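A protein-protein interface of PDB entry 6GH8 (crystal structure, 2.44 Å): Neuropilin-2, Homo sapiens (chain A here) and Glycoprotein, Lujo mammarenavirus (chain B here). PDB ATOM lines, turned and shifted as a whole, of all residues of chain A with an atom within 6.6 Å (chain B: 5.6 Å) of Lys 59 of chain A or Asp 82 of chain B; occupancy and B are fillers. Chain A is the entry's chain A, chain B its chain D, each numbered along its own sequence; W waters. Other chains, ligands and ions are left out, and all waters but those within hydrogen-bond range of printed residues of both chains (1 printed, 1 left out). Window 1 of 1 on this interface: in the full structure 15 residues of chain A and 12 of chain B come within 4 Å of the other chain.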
ATOM      1  N   ILE A  57      20.308   8.113  22.742  1.00  0.00           N
ATOM      2  CA  ILE A  57      20.564   9.546  22.796  1.00  0.00           C
ATOM      3  C   ILE A  57      22.056   9.752  22.994  1.00  0.00           C
ATOM      4  O   ILE A  57      22.680   9.056  23.801  1.00  0.00           O
ATOM      5  CB  ILE A  57      19.746  10.225  23.918  1.00  0.00           C
ATOM      6  CG1 ILE A  57      18.249  10.000  23.691  1.00  0.00           C
ATOM      7  CG2 ILE A  57      20.078  11.700  24.029  1.00  0.00           C
ATOM      8  CD1 ILE A  57      17.361  10.785  24.627  1.00  0.00           C
ATOM      9  N   GLU A  58      22.633  10.693  22.246  1.00  0.00           N
ATOM     10  CA  GLU A  58      24.074  10.907  22.297  1.00  0.00           C
ATOM     11  C   GLU A  58      24.513  11.187  23.724  1.00  0.00           C
ATOM     12  O   GLU A  58      23.952  12.051  24.406  1.00  0.00           O
ATOM     13  CB  GLU A  58      24.497  12.064  21.388  1.00  0.00           C
ATOM     14  CG  GLU A  58      25.757  12.774  21.886  1.00  0.00           C
ATOM     15  CD  GLU A  58      26.199  13.921  20.998  1.00  0.00           C
ATOM     16  OE1 GLU A  58      27.419  14.029  20.743  1.00  0.00           O
ATOM     17  OE2 GLU A  58      25.340  14.702  20.547  1.00  0.00           O
ATOM     18  N   LYS A  59      25.503  10.434  24.182  1.00  0.00           N
ATOM     19  CA  LYS A  59      26.014  10.563  25.534  1.00  0.00           C
ATOM     20  C   LYS A  59      27.299  11.374  25.502  1.00  0.00           C
ATOM     21  O   LYS A  59      28.185  11.116  24.679  1.00  0.00           O
ATOM     22  CB  LYS A  59      26.279   9.194  26.162  1.00  0.00           C
ATOM     23  CG  LYS A  59      27.448   9.185  27.139  1.00  0.00           C
ATOM     24  CD  LYS A  59      27.752   7.786  27.644  1.00  0.00           C
ATOM     25  CE  LYS A  59      28.582   7.026  26.621  1.00  0.00           C
ATOM     26  NZ  LYS A  59      29.567   6.090  27.227  1.00  0.00           N
ATOM     27  N   HIS A  60      27.380  12.369  26.375  1.00  0.00           N
ATOM     28  CA  HIS A  60      28.620  13.089  26.614  1.00  0.00           C
ATOM     29  C   HIS A  60      28.458  13.758  27.967  1.00  0.00           C
ATOM     30  O   HIS A  60      28.483  14.988  28.064  1.00  0.00           O
ATOM     31  CB  HIS A  60      28.903  14.100  25.506  1.00  0.00           C
ATOM     32  CG  HIS A  60      30.336  14.134  25.070  1.00  0.00           C
ATOM     33  ND1 HIS A  60      31.305  14.855  25.736  1.00  0.00           N
ATOM     34  CD2 HIS A  60      30.967  13.515  24.044  1.00  0.00           C
ATOM     35  CE1 HIS A  60      32.467  14.694  25.126  1.00  0.00           C
ATOM     36  NE2 HIS A  60      32.289  13.881  24.100  1.00  0.00           N
ATOM     37  N   ASP A  61      28.276  12.949  29.015  1.00  0.00           N
ATOM     38  CA  ASP A  61      27.704  13.419  30.274  1.00  0.00           C
ATOM     39  C   ASP A  61      26.456  14.262  30.030  1.00  0.00           C
ATOM     40  O   ASP A  61      26.199  15.240  30.735  1.00  0.00           O
ATOM     41  CB  ASP A  61      28.751  14.173  31.092  1.00  0.00           C
ATOM     42  CG  ASP A  61      30.034  13.377  31.237  1.00  0.00           C
ATOM     43  OD1 ASP A  61      29.925  12.166  31.538  1.00  0.00           O
ATOM     44  OD2 ASP A  61      31.136  13.931  31.040  1.00  0.00           O
ATOM     45  N   CYS A  62      25.679  13.861  29.018  1.00  0.00           N
ATOM     46  CA  CYS A  62      24.383  14.458  28.701  1.00  0.00           C
ATOM     47  C   CYS A  62      24.491  15.971  28.519  1.00  0.00           C
ATOM     48  O   CYS A  62      23.628  16.734  28.954  1.00  0.00           O
ATOM     49  CB  CYS A  62      23.356  14.120  29.778  1.00  0.00           C
ATOM     50  SG  CYS A  62      23.064  12.352  30.052  1.00  0.00           S
ATOM     51  N   LYS A  63      25.555  16.418  27.865  1.00  0.00           N
ATOM     52  CA  LYS A  63      25.741  17.850  27.692  1.00  0.00           C
ATOM     53  C   LYS A  63      25.139  18.350  26.382  1.00  0.00           C
ATOM     54  O   LYS A  63      24.811  19.536  26.279  1.00  0.00           O
ATOM     55  CB  LYS A  63      27.231  18.197  27.780  1.00  0.00           C
ATOM     56  CG  LYS A  63      27.508  19.613  28.268  1.00  0.00           C
ATOM     57  CD  LYS A  63      27.647  20.630  27.163  1.00  0.00           C
ATOM     58  CE  LYS A  63      28.182  21.930  27.734  1.00  0.00           C
ATOM     59  NZ  LYS A  63      28.407  22.950  26.679  1.00  0.00           N
ATOM     60  N   TYR A  64      24.975  17.472  25.389  1.00  0.00           N
ATOM     61  CA  TYR A  64      24.537  17.846  24.043  1.00  0.00           C
ATOM     62  C   TYR A  64      23.100  17.404  23.816  1.00  0.00           C
ATOM     63  O   TYR A  64      22.187  18.231  23.804  1.00  0.00           O
ATOM     64  CB  TYR A  64      25.456  17.211  23.001  1.00  0.00           C
ATOM     65  CG  TYR A  64      26.886  17.638  23.118  1.00  0.00           C
ATOM     66  CD1 TYR A  64      27.217  18.961  23.344  1.00  0.00           C
ATOM     67  CD2 TYR A  64      27.904  16.701  23.097  1.00  0.00           C
ATOM     68  CE1 TYR A  64      28.526  19.354  23.476  1.00  0.00           C
ATOM     69  CE2 TYR A  64      29.214  17.081  23.250  1.00  0.00           C
ATOM     70  CZ  TYR A  64      29.523  18.411  23.426  1.00  0.00           C
ATOM     71  OH  TYR A  64      30.835  18.801  23.566  1.00  0.00           O
ATOM     72  N   ASP A  65      22.876  16.109  23.621  1.00  0.00           N
ATOM     73  CA  ASP A  65      21.547  15.543  23.471  1.00  0.00           C
ATOM     74  C   ASP A  65      21.132  14.956  24.809  1.00  0.00           C
ATOM     75  O   ASP A  65      21.925  14.264  25.457  1.00  0.00           O
ATOM     76  CB  ASP A  65      21.531  14.445  22.412  1.00  0.00           C
ATOM     77  CG  ASP A  65      21.731  14.974  21.029  1.00  0.00           C
ATOM     78  OD1 ASP A  65      21.945  16.198  20.894  1.00  0.00           O
ATOM     79  OD2 ASP A  65      21.697  14.168  20.077  1.00  0.00           O
ATOM     80  N   CYS A  84      20.658  10.490  28.989  1.00  0.00           N
ATOM     81  CA  CYS A  84      21.206  10.328  27.651  1.00  0.00           C
ATOM     82  C   CYS A  84      21.817   8.933  27.573  1.00  0.00           C
ATOM     83  O   CYS A  84      21.776   8.168  28.540  1.00  0.00           O
ATOM     84  CB  CYS A  84      22.197  11.454  27.360  1.00  0.00           C
ATOM     85  SG  CYS A  84      23.675  11.380  28.372  1.00  0.00           S
ATOM     86  N   GLY A  85      22.387   8.600  26.420  1.00  0.00           N
ATOM     87  CA  GLY A  85      23.118   7.354  26.300  1.00  0.00           C
ATOM     88  C   GLY A  85      22.326   6.176  25.762  1.00  0.00           C
ATOM     89  O   GLY A  85      21.470   6.329  24.887  1.00  0.00           O
ATOM     90  N   ASN A  86      22.602   4.989  26.304  1.00  0.00           N
ATOM     91  CA  ASN A  86      22.164   3.717  25.742  1.00  0.00           C
ATOM     92  C   ASN A  86      21.049   3.038  26.526  1.00  0.00           C
ATOM     93  O   ASN A  86      20.306   2.243  25.948  1.00  0.00           O
ATOM     94  CB  ASN A  86      23.357   2.752  25.659  1.00  0.00           C
ATOM     95  CG  ASN A  86      23.195   1.719  24.571  1.00  0.00           C
ATOM     96  OD1 ASN A  86      22.907   2.052  23.423  1.00  0.00           O
ATOM     97  ND2 ASN A  86      23.375   0.450  24.927  1.00  0.00           N
ATOM     98  N   ARG A 109      25.715  15.042  15.964  1.00  0.00           N
ATOM     99  CA  ARG A 109      25.381  13.635  15.780  1.00  0.00           C
ATOM    100  C   ARG A 109      24.083  13.287  16.500  1.00  0.00           C
ATOM    101  O   ARG A 109      23.778  13.825  17.567  1.00  0.00           O
ATOM    102  CB  ARG A 109      26.519  12.747  16.298  1.00  0.00           C
ATOM    103  CG  ARG A 109      27.190  13.314  17.540  1.00  0.00           C
ATOM    104  CD  ARG A 109      28.681  13.006  17.589  1.00  0.00           C
ATOM    105  NE  ARG A 109      28.936  11.643  18.055  1.00  0.00           N
ATOM    106  CZ  ARG A 109      29.250  11.316  19.307  1.00  0.00           C
ATOM    107  NH1 ARG A 109      29.458  10.043  19.616  1.00  0.00           N
ATOM    108  NH2 ARG A 109      29.359  12.250  20.241  1.00  0.00           N
ATOM    109  N   PHE B  77      30.323   3.877  14.038  1.00  0.00           N
ATOM    110  CA  PHE B  77      30.703   4.173  15.416  1.00  0.00           C
ATOM    111  C   PHE B  77      29.472   4.620  16.187  1.00  0.00           C
ATOM    112  O   PHE B  77      28.807   5.580  15.769  1.00  0.00           O
ATOM    113  CB  PHE B  77      31.788   5.250  15.465  1.00  0.00           C
ATOM    114  CG  PHE B  77      32.335   5.507  16.844  1.00  0.00           C
ATOM    115  CD1 PHE B  77      33.196   4.597  17.446  1.00  0.00           C
ATOM    116  CD2 PHE B  77      32.004   6.665  17.533  1.00  0.00           C
ATOM    117  CE1 PHE B  77      33.707   4.832  18.717  1.00  0.00           C
ATOM    118  CE2 PHE B  77      32.511   6.907  18.802  1.00  0.00           C
ATOM    119  CZ  PHE B  77      33.365   5.987  19.395  1.00  0.00           C
ATOM    120  N   PRO B  78      29.130   3.969  17.299  1.00  0.00           N
ATOM    121  CA  PRO B  78      27.869   4.285  17.982  1.00  0.00           C
ATOM    122  C   PRO B  78      27.818   5.734  18.443  1.00  0.00           C
ATOM    123  O   PRO B  78      28.798   6.280  18.953  1.00  0.00           O
ATOM    124  CB  PRO B  78      27.869   3.322  19.174  1.00  0.00           C
ATOM    125  CG  PRO B  78      28.717   2.178  18.713  1.00  0.00           C
ATOM    126  CD  PRO B  78      29.821   2.834  17.933  1.00  0.00           C
ATOM    127  N   VAL B  79      26.659   6.362  18.238  1.00  0.00           N
ATOM    128  CA  VAL B  79      26.485   7.743  18.673  1.00  0.00           C
ATOM    129  C   VAL B  79      26.588   7.843  20.189  1.00  0.00           C
ATOM    130  O   VAL B  79      27.100   8.835  20.724  1.00  0.00           O
ATOM    131  CB  VAL B  79      25.147   8.308  18.141  1.00  0.00           C
ATOM    132  CG1 VAL B  79      23.983   7.400  18.518  1.00  0.00           C
ATOM    133  CG2 VAL B  79      24.921   9.724  18.638  1.00  0.00           C
ATOM    134  N   THR B  80      26.155   6.806  20.907  1.00  0.00           N
ATOM    135  CA  THR B  80      26.212   6.805  22.364  1.00  0.00           C
ATOM    136  C   THR B  80      27.540   6.290  22.901  1.00  0.00           C
ATOM    137  O   THR B  80      27.579   5.707  23.989  1.00  0.00           O
ATOM    138  CB  THR B  80      25.060   5.980  22.933  1.00  0.00           C
ATOM    139  OG1 THR B  80      25.403   4.588  22.892  1.00  0.00           O
ATOM    140  CG2 THR B  80      23.792   6.221  22.135  1.00  0.00           C
ATOM    141  N   SER B  81      28.627   6.493  22.164  1.00  0.00           N
ATOM    142  CA  SER B  81      29.979   6.364  22.682  1.00  0.00           C
ATOM    143  C   SER B  81      30.712   7.659  22.385  1.00  0.00           C
ATOM    144  O   SER B  81      30.627   8.177  21.266  1.00  0.00           O
ATOM    145  CB  SER B  81      30.719   5.177  22.058  1.00  0.00           C
ATOM    146  OG  SER B  81      29.910   4.016  22.044  1.00  0.00           O
ATOM    147  N   ASP B  82      31.429   8.179  23.376  1.00  0.00           N
ATOM    148  CA  ASP B  82      32.014   9.501  23.241  1.00  0.00           C
ATOM    149  C   ASP B  82      33.147   9.470  22.227  1.00  0.00           C
ATOM    150  O   ASP B  82      33.778   8.437  21.995  1.00  0.00           O
ATOM    151  CB  ASP B  82      32.532  10.010  24.583  1.00  0.00           C
ATOM    152  CG  ASP B  82      31.429  10.194  25.597  1.00  0.00           C
ATOM    153  OD1 ASP B  82      30.348   9.605  25.401  1.00  0.00           O
ATOM    154  OD2 ASP B  82      31.641  10.930  26.584  1.00  0.00           O
ATOM    155  N   LEU B  83      33.380  10.615  21.596  1.00  0.00           N
ATOM    156  CA  LEU B  83      34.508  10.760  20.685  1.00  0.00           C
ATOM    157  C   LEU B  83      34.929  12.214  20.816  1.00  0.00           C
ATOM    158  O   LEU B  83      34.233  13.108  20.326  1.00  0.00           O
ATOM    159  CB  LEU B  83      34.096  10.393  19.259  1.00  0.00           C
ATOM    160  CG  LEU B  83      35.034  10.279  18.050  1.00  0.00           C
ATOM    161  CD1 LEU B  83      34.233   9.862  16.822  1.00  0.00           C
ATOM    162  CD2 LEU B  83      35.823  11.517  17.756  1.00  0.00           C
ATOM    163  N   LYS B  84      36.078  12.436  21.447  1.00  0.00           N
ATOM    164  CA  LYS B  84      36.507  13.753  21.887  1.00  0.00           C
ATOM    165  C   LYS B  84      37.786  14.174  21.186  1.00  0.00           C
ATOM    166  O   LYS B  84      38.521  13.346  20.643  1.00  0.00           O
ATOM    167  CB  LYS B  84      36.715  13.777  23.410  1.00  0.00           C
ATOM    168  CG  LYS B  84      35.668  12.984  24.169  1.00  0.00           C
ATOM    169  CD  LYS B  84      35.948  12.889  25.653  1.00  0.00           C
ATOM    170  CE  LYS B  84      34.745  12.338  26.390  1.00  0.00           C
ATOM    171  NZ  LYS B  84      34.656  12.809  27.800  1.00  0.00           N
ATOM    172  N   GLU B  95      40.504  10.926  20.488  1.00  0.00           N
ATOM    173  CA  GLU B  95      40.283   9.848  21.448  1.00  0.00           C
ATOM    174  C   GLU B  95      38.908   9.230  21.250  1.00  0.00           C
ATOM    175  O   GLU B  95      37.894   9.930  21.303  1.00  0.00           O
ATOM    176  CB  GLU B  95      40.433  10.359  22.885  1.00  0.00           C
ATOM    177  CG  GLU B  95      39.562   9.636  23.903  1.00  0.00           C
ATOM    178  CD  GLU B  95      39.658  10.233  25.297  1.00  0.00           C
ATOM    179  OE1 GLU B  95      40.703  10.833  25.626  1.00  0.00           O
ATOM    180  OE2 GLU B  95      38.681  10.100  26.067  1.00  0.00           O
ATOM    181  N   TYR B  96      38.885   7.925  20.996  1.00  0.00           N
ATOM    182  CA  TYR B  96      37.660   7.143  21.001  1.00  0.00           C
ATOM    183  C   TYR B  96      37.399   6.599  22.403  1.00  0.00           C
ATOM    184  O   TYR B  96      38.301   6.506  23.240  1.00  0.00           O
ATOM    185  CB  TYR B  96      37.742   5.975  20.018  1.00  0.00           C
ATOM    186  CG  TYR B  96      37.776   6.350  18.553  1.00  0.00           C
ATOM    187  CD1 TYR B  96      36.613   6.673  17.864  1.00  0.00           C
ATOM    188  CD2 TYR B  96      38.972   6.343  17.850  1.00  0.00           C
ATOM    189  CE1 TYR B  96      36.649   6.997  16.518  1.00  0.00           C
ATOM    190  CE2 TYR B  96      39.018   6.661  16.512  1.00  0.00           C
ATOM    191  CZ  TYR B  96      37.856   6.989  15.850  1.00  0.00           C
ATOM    192  OH  TYR B  96      37.909   7.305  14.518  1.00  0.00           O
ATOM    193  N   GLU B  97      36.150   6.224  22.647  1.00  0.00           N
ATOM    194  CA  GLU B  97      35.761   5.545  23.875  1.00  0.00           C
ATOM    195  C   GLU B  97      35.420   4.104  23.527  1.00  0.00           C
ATOM    196  O   GLU B  97      34.586   3.862  22.648  1.00  0.00           O
ATOM    197  CB  GLU B  97      34.561   6.231  24.528  1.00  0.00           C
ATOM    198  CG  GLU B  97      33.870   5.365  25.550  1.00  0.00           C
ATOM    199  CD  GLU B  97      32.735   6.072  26.253  1.00  0.00           C
ATOM    200  OE1 GLU B  97      31.672   6.246  25.626  1.00  0.00           O
ATOM    201  OE2 GLU B  97      32.911   6.468  27.425  1.00  0.00           O
ATOM    202  N   THR B  99      33.596   0.926  24.324  1.00  0.00           N
ATOM    203  CA  THR B  99      32.453   0.413  25.073  1.00  0.00           C
ATOM    204  C   THR B  99      32.084  -0.968  24.540  1.00  0.00           C
ATOM    205  O   THR B  99      32.728  -1.499  23.632  1.00  0.00           O
ATOM    206  CB  THR B  99      31.246   1.359  24.981  1.00  0.00           C
ATOM    207  OG1 THR B  99      30.653   1.266  23.677  1.00  0.00           O
ATOM    208  CG2 THR B  99      31.650   2.793  25.240  1.00  0.00           C
HETATM  209  O   HOH W   1      30.211  10.631  28.544  1.00  0.00           O
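OG of Ser 81 of chain B lies within hydrogen-bond range of OG1 of Thr 99 of chain B (3.3 Å).
NZ of Lys 84 of chain B lies within salt-bridge range of OD2 of Asp 82 of chain B, at 3.8 Å.
The backbone NH of Asp 82 of chain B sits at hydrogen-bond distance from the side-chain carboxylate of Glu 97 of chain B.
N of Lys 84 of chain B sits at hydrogen-bond distance from O of Glu 95 of chain B.
O of Ile 57 of chain A is in hydrogen-bond range of N of Gly 85 of chain A (2.7 Å).
SG of Cys 62 of chain A is disulfide-bonded to SG of Cys 84 of chain A, at 2.0 Å.
Lys 59 of chain A touches three residues of chain B.
Asp 82 of chain B touches just these residues of chain A: Lys 59 and His 60.
Of the printed residues of chain B, Asn 86 of chain A touches Thr 80 (3.6 Å).
Of the printed residues of chain B, Glu 58 of chain A touches Val 79.
The nearest residue of chain A that does not touch Asp 82 of chain B is Arg 109 of chain A (4.5 Å).
O of Val 79 of chain B sits at hydrogen-bond distance from NH1 of Arg 109 of chain A, 2.9 Å away.
O of Ser 81 of chain B is in hydrogen-bond range of NH1 of Arg 109 of chain A, 2.8 Å away.
The backbone carbonyl oxygen of Lys 59 of chain A sits close to the side-chain carboxylate of Asp 82 of chain B (2.7 Å).
OE1 of Glu 97 of chain B lies within salt-bridge range of NZ of Lys 59 of chain A, at 2.6 Å.
Among the printed residues, merely in contact across the chains: Lys 59 of chain A with Thr 80 of chain B (3.1 Å), Ile 57 of chain A with Thr 80 of chain B (3.5 Å), His 60 of chain A with Lys 84 of chain B (3.5 Å), Asn 86 of chain A with Thr 80 of chain B (3.6 Å), Gly 85 of chain A with Thr 80 of chain B (3.6 Å), Glu 58 of chain A with Val 79 of chain B (3.6 Å), His 60 of chain A with Asp 82 of chain B (3.7 Å) and Arg 109 of chain A with Pro 78 of chain B (3.9 Å).
Of the 13 printed residues of chain A, 7 touch a printed residue of chain B.
Hydrophobic or aromatic side chains of chain A within 4 Å of the printed part of chain B: His 60.
Of the 12 printed residues of chain B, 7 touch a printed residue of chain A.
Printed residues of chain B that touch a printed residue of chain A: Pro 78, Val 79, Thr 80, Ser 81, Asp 82, Lys 84 and Glu 97.
Hydrophobic or aromatic side chains of chain B within 4 Å of the printed part of chain A: Val 79.
Among the printed residues, Asp or Glu carboxylates within 4 Å of a Lys or Arg side-chain nitrogen of the other chain: Lys 59 of chain A with Glu 97 of chain B (2.6 Å).
Water W1 bridges OD2 of Asp 82 of chain B (2.4 Å) and N of Asp 61 of chain A (3.1 Å).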
